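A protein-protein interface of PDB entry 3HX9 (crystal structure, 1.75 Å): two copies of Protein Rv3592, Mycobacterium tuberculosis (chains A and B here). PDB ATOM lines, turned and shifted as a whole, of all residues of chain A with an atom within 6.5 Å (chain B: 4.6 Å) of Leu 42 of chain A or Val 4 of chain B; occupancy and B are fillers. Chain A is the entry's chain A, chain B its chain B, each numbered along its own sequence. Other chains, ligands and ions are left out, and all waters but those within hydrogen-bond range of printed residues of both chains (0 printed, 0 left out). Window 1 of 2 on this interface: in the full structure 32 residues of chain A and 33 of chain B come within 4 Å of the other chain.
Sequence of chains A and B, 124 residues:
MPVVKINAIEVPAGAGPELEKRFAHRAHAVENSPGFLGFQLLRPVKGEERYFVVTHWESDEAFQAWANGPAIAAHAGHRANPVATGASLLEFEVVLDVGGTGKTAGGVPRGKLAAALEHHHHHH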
ATOM      1  N   GLN A  40      -3.647  28.703 -21.581  1.00  0.00           N
ATOM      2  CA  GLN A  40      -4.072  27.344 -21.399  1.00  0.00           C
ATOM      3  C   GLN A  40      -3.399  26.819 -20.184  1.00  0.00           C
ATOM      4  O   GLN A  40      -2.225  27.154 -19.932  1.00  0.00           O
ATOM      5  CB  GLN A  40      -3.632  26.427 -22.569  1.00  0.00           C
ATOM      6  CG  GLN A  40      -4.293  26.835 -23.921  1.00  0.00           C
ATOM      7  CD  GLN A  40      -3.639  28.045 -24.557  1.00  0.00           C
ATOM      8  OE1 GLN A  40      -2.380  28.125 -24.625  1.00  0.00           O
ATOM      9  NE2 GLN A  40      -4.457  29.001 -25.064  1.00  0.00           N
ATOM     10  N   LEU A  41      -4.080  25.917 -19.507  1.00  0.00           N
ATOM     11  CA  LEU A  41      -3.391  25.084 -18.450  1.00  0.00           C
ATOM     12  C   LEU A  41      -3.178  23.698 -19.087  1.00  0.00           C
ATOM     13  O   LEU A  41      -4.121  23.063 -19.539  1.00  0.00           O
ATOM     14  CB  LEU A  41      -4.254  24.938 -17.189  1.00  0.00           C
ATOM     15  CG  LEU A  41      -3.678  24.021 -16.091  1.00  0.00           C
ATOM     16  CD1 LEU A  41      -2.423  24.716 -15.503  1.00  0.00           C
ATOM     17  CD2 LEU A  41      -4.697  23.890 -14.983  1.00  0.00           C
ATOM     18  N   LEU A  42      -1.919  23.275 -19.128  1.00  0.00           N
ATOM     19  CA  LEU A  42      -1.530  21.994 -19.701  1.00  0.00           C
ATOM     20  C   LEU A  42      -1.108  21.037 -18.575  1.00  0.00           C
ATOM     21  O   LEU A  42      -0.130  21.264 -17.821  1.00  0.00           O
ATOM     22  CB  LEU A  42      -0.344  22.216 -20.657  1.00  0.00           C
ATOM     23  CG  LEU A  42      -0.655  23.272 -21.769  1.00  0.00           C
ATOM     24  CD1 LEU A  42       0.516  23.144 -22.803  1.00  0.00           C
ATOM     25  CD2 LEU A  42      -1.983  22.874 -22.503  1.00  0.00           C
ATOM     26  N   ARG A  43      -1.811  19.918 -18.542  1.00  0.00           N
ATOM     27  CA  ARG A  43      -1.489  18.834 -17.599  1.00  0.00           C
ATOM     28  C   ARG A  43      -0.427  17.882 -18.200  1.00  0.00           C
ATOM     29  O   ARG A  43      -0.590  17.405 -19.287  1.00  0.00           O
ATOM     30  CB  ARG A  43      -2.794  18.078 -17.280  1.00  0.00           C
ATOM     31  CG  ARG A  43      -2.553  16.908 -16.300  1.00  0.00           C
ATOM     32  CD  ARG A  43      -3.927  16.608 -15.598  1.00  0.00           C
ATOM     33  NE  ARG A  43      -4.671  16.044 -16.625  1.00  0.00           N
ATOM     34  CZ  ARG A  43      -5.940  16.216 -17.006  1.00  0.00           C
ATOM     35  NH1 ARG A  43      -6.902  16.871 -16.378  1.00  0.00           N
ATOM     36  NH2 ARG A  43      -6.257  15.567 -18.122  1.00  0.00           N
ATOM     37  N   PRO A  44       0.675  17.617 -17.490  1.00  0.00           N
ATOM     38  CA  PRO A  44       1.753  16.824 -18.080  1.00  0.00           C
ATOM     39  C   PRO A  44       1.366  15.345 -18.204  1.00  0.00           C
ATOM     40  O   PRO A  44       0.695  14.782 -17.297  1.00  0.00           O
ATOM     41  CB  PRO A  44       2.900  16.991 -17.079  1.00  0.00           C
ATOM     42  CG  PRO A  44       2.265  17.322 -15.792  1.00  0.00           C
ATOM     43  CD  PRO A  44       0.976  18.089 -16.106  1.00  0.00           C
ATOM     44  N   ARG A  50       6.023  18.929 -14.909  1.00  0.00           N
ATOM     45  CA  ARG A  50       5.440  20.221 -14.482  1.00  0.00           C
ATOM     46  C   ARG A  50       4.168  20.480 -15.287  1.00  0.00           C
ATOM     47  O   ARG A  50       4.074  20.035 -16.427  1.00  0.00           O
ATOM     48  CB  ARG A  50       6.396  21.381 -14.738  1.00  0.00           C
ATOM     49  CG  ARG A  50       7.714  21.149 -13.987  1.00  0.00           C
ATOM     50  CD  ARG A  50       8.713  22.271 -14.255  1.00  0.00           C
ATOM     51  NE  ARG A  50       9.215  22.122 -15.601  1.00  0.00           N
ATOM     52  CZ  ARG A  50      10.118  22.936 -16.129  1.00  0.00           C
ATOM     53  NH1 ARG A  50      10.592  23.977 -15.400  1.00  0.00           N
ATOM     54  NH2 ARG A  50      10.544  22.704 -17.385  1.00  0.00           N
ATOM     55  N   TYR A  51       3.225  21.139 -14.658  1.00  0.00           N
ATOM     56  CA  TYR A  51       2.120  21.765 -15.439  1.00  0.00           C
ATOM     57  C   TYR A  51       2.697  22.963 -16.176  1.00  0.00           C
ATOM     58  O   TYR A  51       3.563  23.668 -15.643  1.00  0.00           O
ATOM     59  CB  TYR A  51       1.023  22.261 -14.524  1.00  0.00           C
ATOM     60  CG  TYR A  51       0.042  21.187 -14.109  1.00  0.00           C
ATOM     61  CD1 TYR A  51      -1.285  21.157 -14.628  1.00  0.00           C
ATOM     62  CD2 TYR A  51       0.432  20.222 -13.206  1.00  0.00           C
ATOM     63  CE1 TYR A  51      -2.179  20.130 -14.244  1.00  0.00           C
ATOM     64  CE2 TYR A  51      -0.465  19.189 -12.802  1.00  0.00           C
ATOM     65  CZ  TYR A  51      -1.753  19.198 -13.284  1.00  0.00           C
ATOM     66  OH  TYR A  51      -2.608  18.174 -12.862  1.00  0.00           O
ATOM     67  N   PHE A  52       2.174  23.231 -17.377  1.00  0.00           N
ATOM     68  CA  PHE A  52       2.579  24.464 -18.107  1.00  0.00           C
ATOM     69  C   PHE A  52       1.386  25.372 -18.174  1.00  0.00           C
ATOM     70  O   PHE A  52       0.334  24.947 -18.649  1.00  0.00           O
ATOM     71  CB  PHE A  52       2.996  24.167 -19.571  1.00  0.00           C
ATOM     72  CG  PHE A  52       4.422  23.731 -19.762  1.00  0.00           C
ATOM     73  CD1 PHE A  52       5.204  23.329 -18.667  1.00  0.00           C
ATOM     74  CD2 PHE A  52       4.990  23.715 -21.026  1.00  0.00           C
ATOM     75  CE1 PHE A  52       6.520  22.935 -18.861  1.00  0.00           C
ATOM     76  CE2 PHE A  52       6.310  23.313 -21.243  1.00  0.00           C
ATOM     77  CZ  PHE A  52       7.057  22.876 -20.112  1.00  0.00           C
ATOM     78  N   VAL A  53       1.548  26.602 -17.690  1.00  0.00           N
ATOM     79  CA  VAL A  53       0.527  27.603 -17.737  1.00  0.00           C
ATOM     80  C   VAL A  53       0.976  28.504 -18.888  1.00  0.00           C
ATOM     81  O   VAL A  53       1.900  29.276 -18.734  1.00  0.00           O
ATOM     82  CB  VAL A  53       0.458  28.381 -16.425  1.00  0.00           C
ATOM     83  CG1 VAL A  53      -0.636  29.471 -16.482  1.00  0.00           C
ATOM     84  CG2 VAL A  53       0.075  27.331 -15.303  1.00  0.00           C
ATOM     85  N   VAL A  54       0.382  28.288 -20.042  1.00  0.00           N
ATOM     86  CA  VAL A  54       0.860  28.881 -21.321  1.00  0.00           C
ATOM     87  C   VAL A  54       0.063  30.147 -21.575  1.00  0.00           C
ATOM     88  O   VAL A  54      -1.132  30.073 -21.923  1.00  0.00           O
ATOM     89  CB  VAL A  54       0.685  27.904 -22.476  1.00  0.00           C
ATOM     90  CG1 VAL A  54       1.204  28.533 -23.811  1.00  0.00           C
ATOM     91  CG2 VAL A  54       1.390  26.605 -22.175  1.00  0.00           C
ATOM     92  N   PRO B   2      -8.448  18.285 -26.069  1.00  0.00           N
ATOM     93  CA  PRO B   2      -7.263  18.314 -26.994  1.00  0.00           C
ATOM     94  C   PRO B   2      -5.954  18.130 -26.254  1.00  0.00           C
ATOM     95  O   PRO B   2      -5.925  18.002 -25.015  1.00  0.00           O
ATOM     96  CB  PRO B   2      -7.305  19.691 -27.638  1.00  0.00           C
ATOM     97  CG  PRO B   2      -8.594  20.345 -27.194  1.00  0.00           C
ATOM     98  CD  PRO B   2      -9.230  19.541 -26.127  1.00  0.00           C
ATOM     99  N   VAL B   3      -4.896  17.947 -27.036  1.00  0.00           N
ATOM    100  CA  VAL B   3      -3.581  17.676 -26.401  1.00  0.00           C
ATOM    101  C   VAL B   3      -2.597  18.583 -27.028  1.00  0.00           C
ATOM    102  O   VAL B   3      -2.828  19.087 -28.109  1.00  0.00           O
ATOM    103  CB  VAL B   3      -3.097  16.210 -26.603  1.00  0.00           C
ATOM    104  CG1 VAL B   3      -4.102  15.260 -25.988  1.00  0.00           C
ATOM    105  CG2 VAL B   3      -3.010  15.771 -28.112  1.00  0.00           C
ATOM    106  N   VAL B   4      -1.435  18.717 -26.382  1.00  0.00           N
ATOM    107  CA  VAL B   4      -0.322  19.559 -26.921  1.00  0.00           C
ATOM    108  C   VAL B   4       0.875  18.670 -26.895  1.00  0.00           C
ATOM    109  O   VAL B   4       1.132  17.998 -25.876  1.00  0.00           O
ATOM    110  CB  VAL B   4      -0.093  20.790 -25.994  1.00  0.00           C
ATOM    111  CG1 VAL B   4       1.211  21.486 -26.334  1.00  0.00           C
ATOM    112  CG2 VAL B   4      -1.228  21.777 -26.212  1.00  0.00           C
ATOM    113  N   LYS B   5       1.580  18.634 -28.018  1.00  0.00           N
ATOM    114  CA  LYS B   5       2.830  17.871 -28.114  1.00  0.00           C
ATOM    115  C   LYS B   5       3.901  18.876 -28.488  1.00  0.00           C
ATOM    116  O   LYS B   5       3.843  19.475 -29.565  1.00  0.00           O
ATOM    117  CB  LYS B   5       2.665  16.776 -29.163  1.00  0.00           C
ATOM    118  CG  LYS B   5       1.395  15.898 -28.933  1.00  0.00           C
ATOM    119  CD  LYS B   5       1.587  14.923 -27.751  1.00  0.00           C
ATOM    120  CE  LYS B   5       0.422  13.881 -27.717  1.00  0.00           C
ATOM    121  NZ  LYS B   5       0.506  12.986 -26.504  1.00  0.00           N
ATOM    122  N   ILE B   6       4.921  19.054 -27.626  1.00  0.00           N
ATOM    123  CA  ILE B   6       5.885  20.124 -27.904  1.00  0.00           C
ATOM    124  C   ILE B   6       7.196  19.385 -28.213  1.00  0.00           C
ATOM    125  O   ILE B   6       7.606  18.555 -27.362  1.00  0.00           O
ATOM    126  CB  ILE B   6       6.111  20.955 -26.625  1.00  0.00           C
ATOM    127  CG1 ILE B   6       4.799  21.601 -26.185  1.00  0.00           C
ATOM    128  CG2 ILE B   6       7.270  22.057 -26.847  1.00  0.00           C
ATOM    129  CD1 ILE B   6       4.935  22.634 -25.061  1.00  0.00           C
ATOM    130  N   VAL B  54       5.413  23.859 -30.804  1.00  0.00           N
ATOM    131  CA  VAL B  54       4.191  23.572 -30.019  1.00  0.00           C
ATOM    132  C   VAL B  54       3.115  23.112 -30.972  1.00  0.00           C
ATOM    133  O   VAL B  54       2.579  23.946 -31.709  1.00  0.00           O
ATOM    134  CB  VAL B  54       3.720  24.848 -29.298  1.00  0.00           C
ATOM    135  CG1 VAL B  54       2.490  24.579 -28.429  1.00  0.00           C
ATOM    136  CG2 VAL B  54       4.848  25.379 -28.445  1.00  0.00           C
ATOM    137  N   THR B  55       2.811  21.823 -30.947  1.00  0.00           N
ATOM    138  CA  THR B  55       1.804  21.295 -31.915  1.00  0.00           C
ATOM    139  C   THR B  55       0.535  20.945 -31.159  1.00  0.00           C
ATOM    140  O   THR B  55       0.573  20.528 -29.981  1.00  0.00           O
ATOM    141  CB  THR B  55       2.259  20.085 -32.705  1.00  0.00           C
ATOM    142  OG1 THR B  55       2.296  18.929 -31.851  1.00  0.00           O
ATOM    143  CG2 THR B  55       3.652  20.294 -33.338  1.00  0.00           C
ATOM    144  N   HIS B  56      -0.596  21.122 -31.861  1.00  0.00           N
ATOM    145  CA  HIS B  56      -1.937  20.965 -31.228  1.00  0.00           C
ATOM    146  C   HIS B  56      -2.728  19.879 -31.952  1.00  0.00           C
ATOM    147  O   HIS B  56      -2.764  19.869 -33.177  1.00  0.00           O
ATOM    148  CB  HIS B  56      -2.696  22.303 -31.360  1.00  0.00           C
ATOM    149  CG  HIS B  56      -2.049  23.408 -30.562  1.00  0.00           C
ATOM    150  ND1 HIS B  56      -1.083  24.250 -31.047  1.00  0.00           N
ATOM    151  CD2 HIS B  56      -2.196  23.716 -29.251  1.00  0.00           C
ATOM    152  CE1 HIS B  56      -0.685  25.062 -30.075  1.00  0.00           C
ATOM    153  NE2 HIS B  56      -1.387  24.797 -28.998  1.00  0.00           N
ATOM    154  N   LEU B  90       7.612  16.802 -25.251  1.00  0.00           N
ATOM    155  CA  LEU B  90       6.940  17.092 -23.999  1.00  0.00           C
ATOM    156  C   LEU B  90       5.454  16.955 -24.325  1.00  0.00           C
ATOM    157  O   LEU B  90       4.985  17.574 -25.295  1.00  0.00           O
ATOM    158  CB  LEU B  90       7.249  18.537 -23.478  1.00  0.00           C
ATOM    159  CG  LEU B  90       8.709  18.934 -23.675  1.00  0.00           C
ATOM    160  CD1 LEU B  90       8.910  20.426 -23.250  1.00  0.00           C
ATOM    161  CD2 LEU B  90       9.624  17.972 -22.838  1.00  0.00           C
ATOM    162  N   GLU B  91       4.757  16.116 -23.555  1.00  0.00           N
ATOM    163  CA  GLU B  91       3.366  15.826 -23.936  1.00  0.00           C
ATOM    164  C   GLU B  91       2.381  16.180 -22.864  1.00  0.00           C
ATOM    165  O   GLU B  91       2.567  15.847 -21.672  1.00  0.00           O
ATOM    166  CB  GLU B  91       3.196  14.317 -24.248  1.00  0.00           C
ATOM    167  CG  GLU B  91       4.294  13.786 -25.180  1.00  0.00           C
ATOM    168  CD  GLU B  91       4.026  12.337 -25.611  1.00  0.00           C
ATOM    169  OE1 GLU B  91       2.870  11.946 -25.945  1.00  0.00           O
ATOM    170  OE2 GLU B  91       5.025  11.594 -25.654  1.00  0.00           O
ATOM    171  N   PHE B  92       1.282  16.815 -23.280  1.00  0.00           N
ATOM    172  CA  PHE B  92       0.374  17.346 -22.295  1.00  0.00           C
ATOM    173  C   PHE B  92      -1.073  17.150 -22.731  1.00  0.00           C
ATOM    174  O   PHE B  92      -1.331  16.966 -23.894  1.00  0.00           O
ATOM    175  CB  PHE B  92       0.504  18.883 -22.139  1.00  0.00           C
ATOM    176  CG  PHE B  92       1.866  19.355 -21.719  1.00  0.00           C
ATOM    177  CD1 PHE B  92       2.139  19.554 -20.363  1.00  0.00           C
ATOM    178  CD2 PHE B  92       2.856  19.616 -22.671  1.00  0.00           C
ATOM    179  CE1 PHE B  92       3.413  20.040 -19.935  1.00  0.00           C
ATOM    180  CE2 PHE B  92       4.152  20.089 -22.228  1.00  0.00           C
ATOM    181  CZ  PHE B  92       4.401  20.286 -20.882  1.00  0.00           C
ATOM    182  N   GLU B  93      -1.972  17.283 -21.765  1.00  0.00           N
ATOM    183  CA  GLU B  93      -3.409  17.341 -22.042  1.00  0.00           C
ATOM    184  C   GLU B  93      -3.926  18.721 -21.704  1.00  0.00           C
ATOM    185  O   GLU B  93      -3.558  19.325 -20.711  1.00  0.00           O
ATOM    186  CB  GLU B  93      -4.162  16.291 -21.198  1.00  0.00           C
ATOM    187  CG  GLU B  93      -3.951  14.831 -21.673  1.00  0.00           C
ATOM    188  CD  GLU B  93      -4.425  13.752 -20.682  1.00  0.00           C
ATOM    189  OE1 GLU B  93      -4.739  14.078 -19.514  1.00  0.00           O
ATOM    190  OE2 GLU B  93      -4.399  12.549 -21.078  1.00  0.00           O
ATOM    191  N   VAL B  94      -4.814  19.266 -22.515  1.00  0.00           N
ATOM    192  CA  VAL B  94      -5.280  20.591 -22.244  1.00  0.00           C
ATOM    193  C   VAL B  94      -6.414  20.540 -21.186  1.00  0.00           C
ATOM    194  O   VAL B  94      -7.451  19.875 -21.400  1.00  0.00           O
ATOM    195  CB  VAL B  94      -5.807  21.264 -23.541  1.00  0.00           C
ATOM    196  CG1 VAL B  94      -6.388  22.670 -23.188  1.00  0.00           C
ATOM    197  CG2 VAL B  94      -4.729  21.377 -24.594  1.00  0.00           C
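NH2 of Arg 43 of chain A is in salt-bridge range of OE1 of Glu 93 of chain B (2.5 Å).
N of Leu 42 of chain A is in hydrogen-bond range of O of Phe 52 of chain A. N of Val 94 of chain B sits at hydrogen-bond distance from O of Pro 2 of chain B (3.0 Å). The backbone NH of Phe 92 of chain B sits at hydrogen-bond distance from the backbone carbonyl oxygen of Val 4 of chain B. The side-chain carboxylate of Glu 91 of chain B is in salt-bridge range of the side-chain amino group of Lys 5 of chain B (2.6 Å).
Among the printed residues, merely in contact across the chains: Arg 43 of chain A with Phe 92 of chain B (3.2 Å), Phe 52 of chain A with Phe 92 of chain B (3.5 Å), Leu 42 of chain A with Glu 93 of chain B (3.5 Å), Arg 50 of chain A with Phe 92 of chain B (3.6 Å), Pro 44 of chain A with Phe 92 of chain B (3.6 Å), Leu 42 of chain A with Phe 92 of chain B (3.7 Å), Pro 44 of chain A with Glu 91 of chain B (3.7 Å), Leu 42 of chain A with Val 94 of chain B (3.8 Å), Leu 41 of chain A with Val 94 of chain B (3.8 Å), Leu 42 of chain A with Val 4 of chain B (3.9 Å) and Leu 41 of chain A with Glu 93 of chain B (3.96 Å).
Of chain B, only Val 4, Phe 92, Glu 93 and Val 94 come within 4 Å of Leu 42 of chain A. Val 4 of chain B touches just one residue of chain A: Leu 42 (3.9 Å). Of the printed residues of chain B, Arg 50 of chain A touches Phe 92 (3.6 Å). Of the printed residues of chain B, Leu 41 of chain A touches Glu 93 (3.96 Å) and Val 94 (3.8 Å). Of the printed residues of chain A, Phe 92 of chain B touches Leu 42 (3.7 Å), Arg 43 (3.2 Å), Pro 44 (3.6 Å), Arg 50 (3.6 Å) and Phe 52 (3.5 Å). Of the printed residues of chain A, Val 94 of chain B touches Leu 41 (3.8 Å) and Leu 42 (3.8 Å). The nearest printed residue of chain B that does not touch Leu 42 of chain A is Ile 6 of chain B (5.0 Å). The nearest printed residue of chain A that does not touch Glu 93 of chain B is Pro 44 of chain A (5.0 Å).
Hydrophobic or aromatic side chains of chain A that line the printed part of chain B: Leu 42 and Phe 52. Along chain A the printed residues that touch a printed residue of chain B span positions 41 to 52. Printed residues of chain B that touch a printed residue of chain A: Val 4, Glu 91, Phe 92, Glu 93 and Val 94. Hydrophobic or aromatic side chains of chain B within 4 Å of the printed part of chain A: Val 4, Phe 92 and Val 94. Among the printed residues, 12 pairs touch across the chains. Among the printed residues, Asp or Glu carboxylates within 4 Å of a Lys or Arg side-chain nitrogen of the other chain: Arg 43 of chain A with Glu 93 of chain B.
1 position is printed for both chains.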
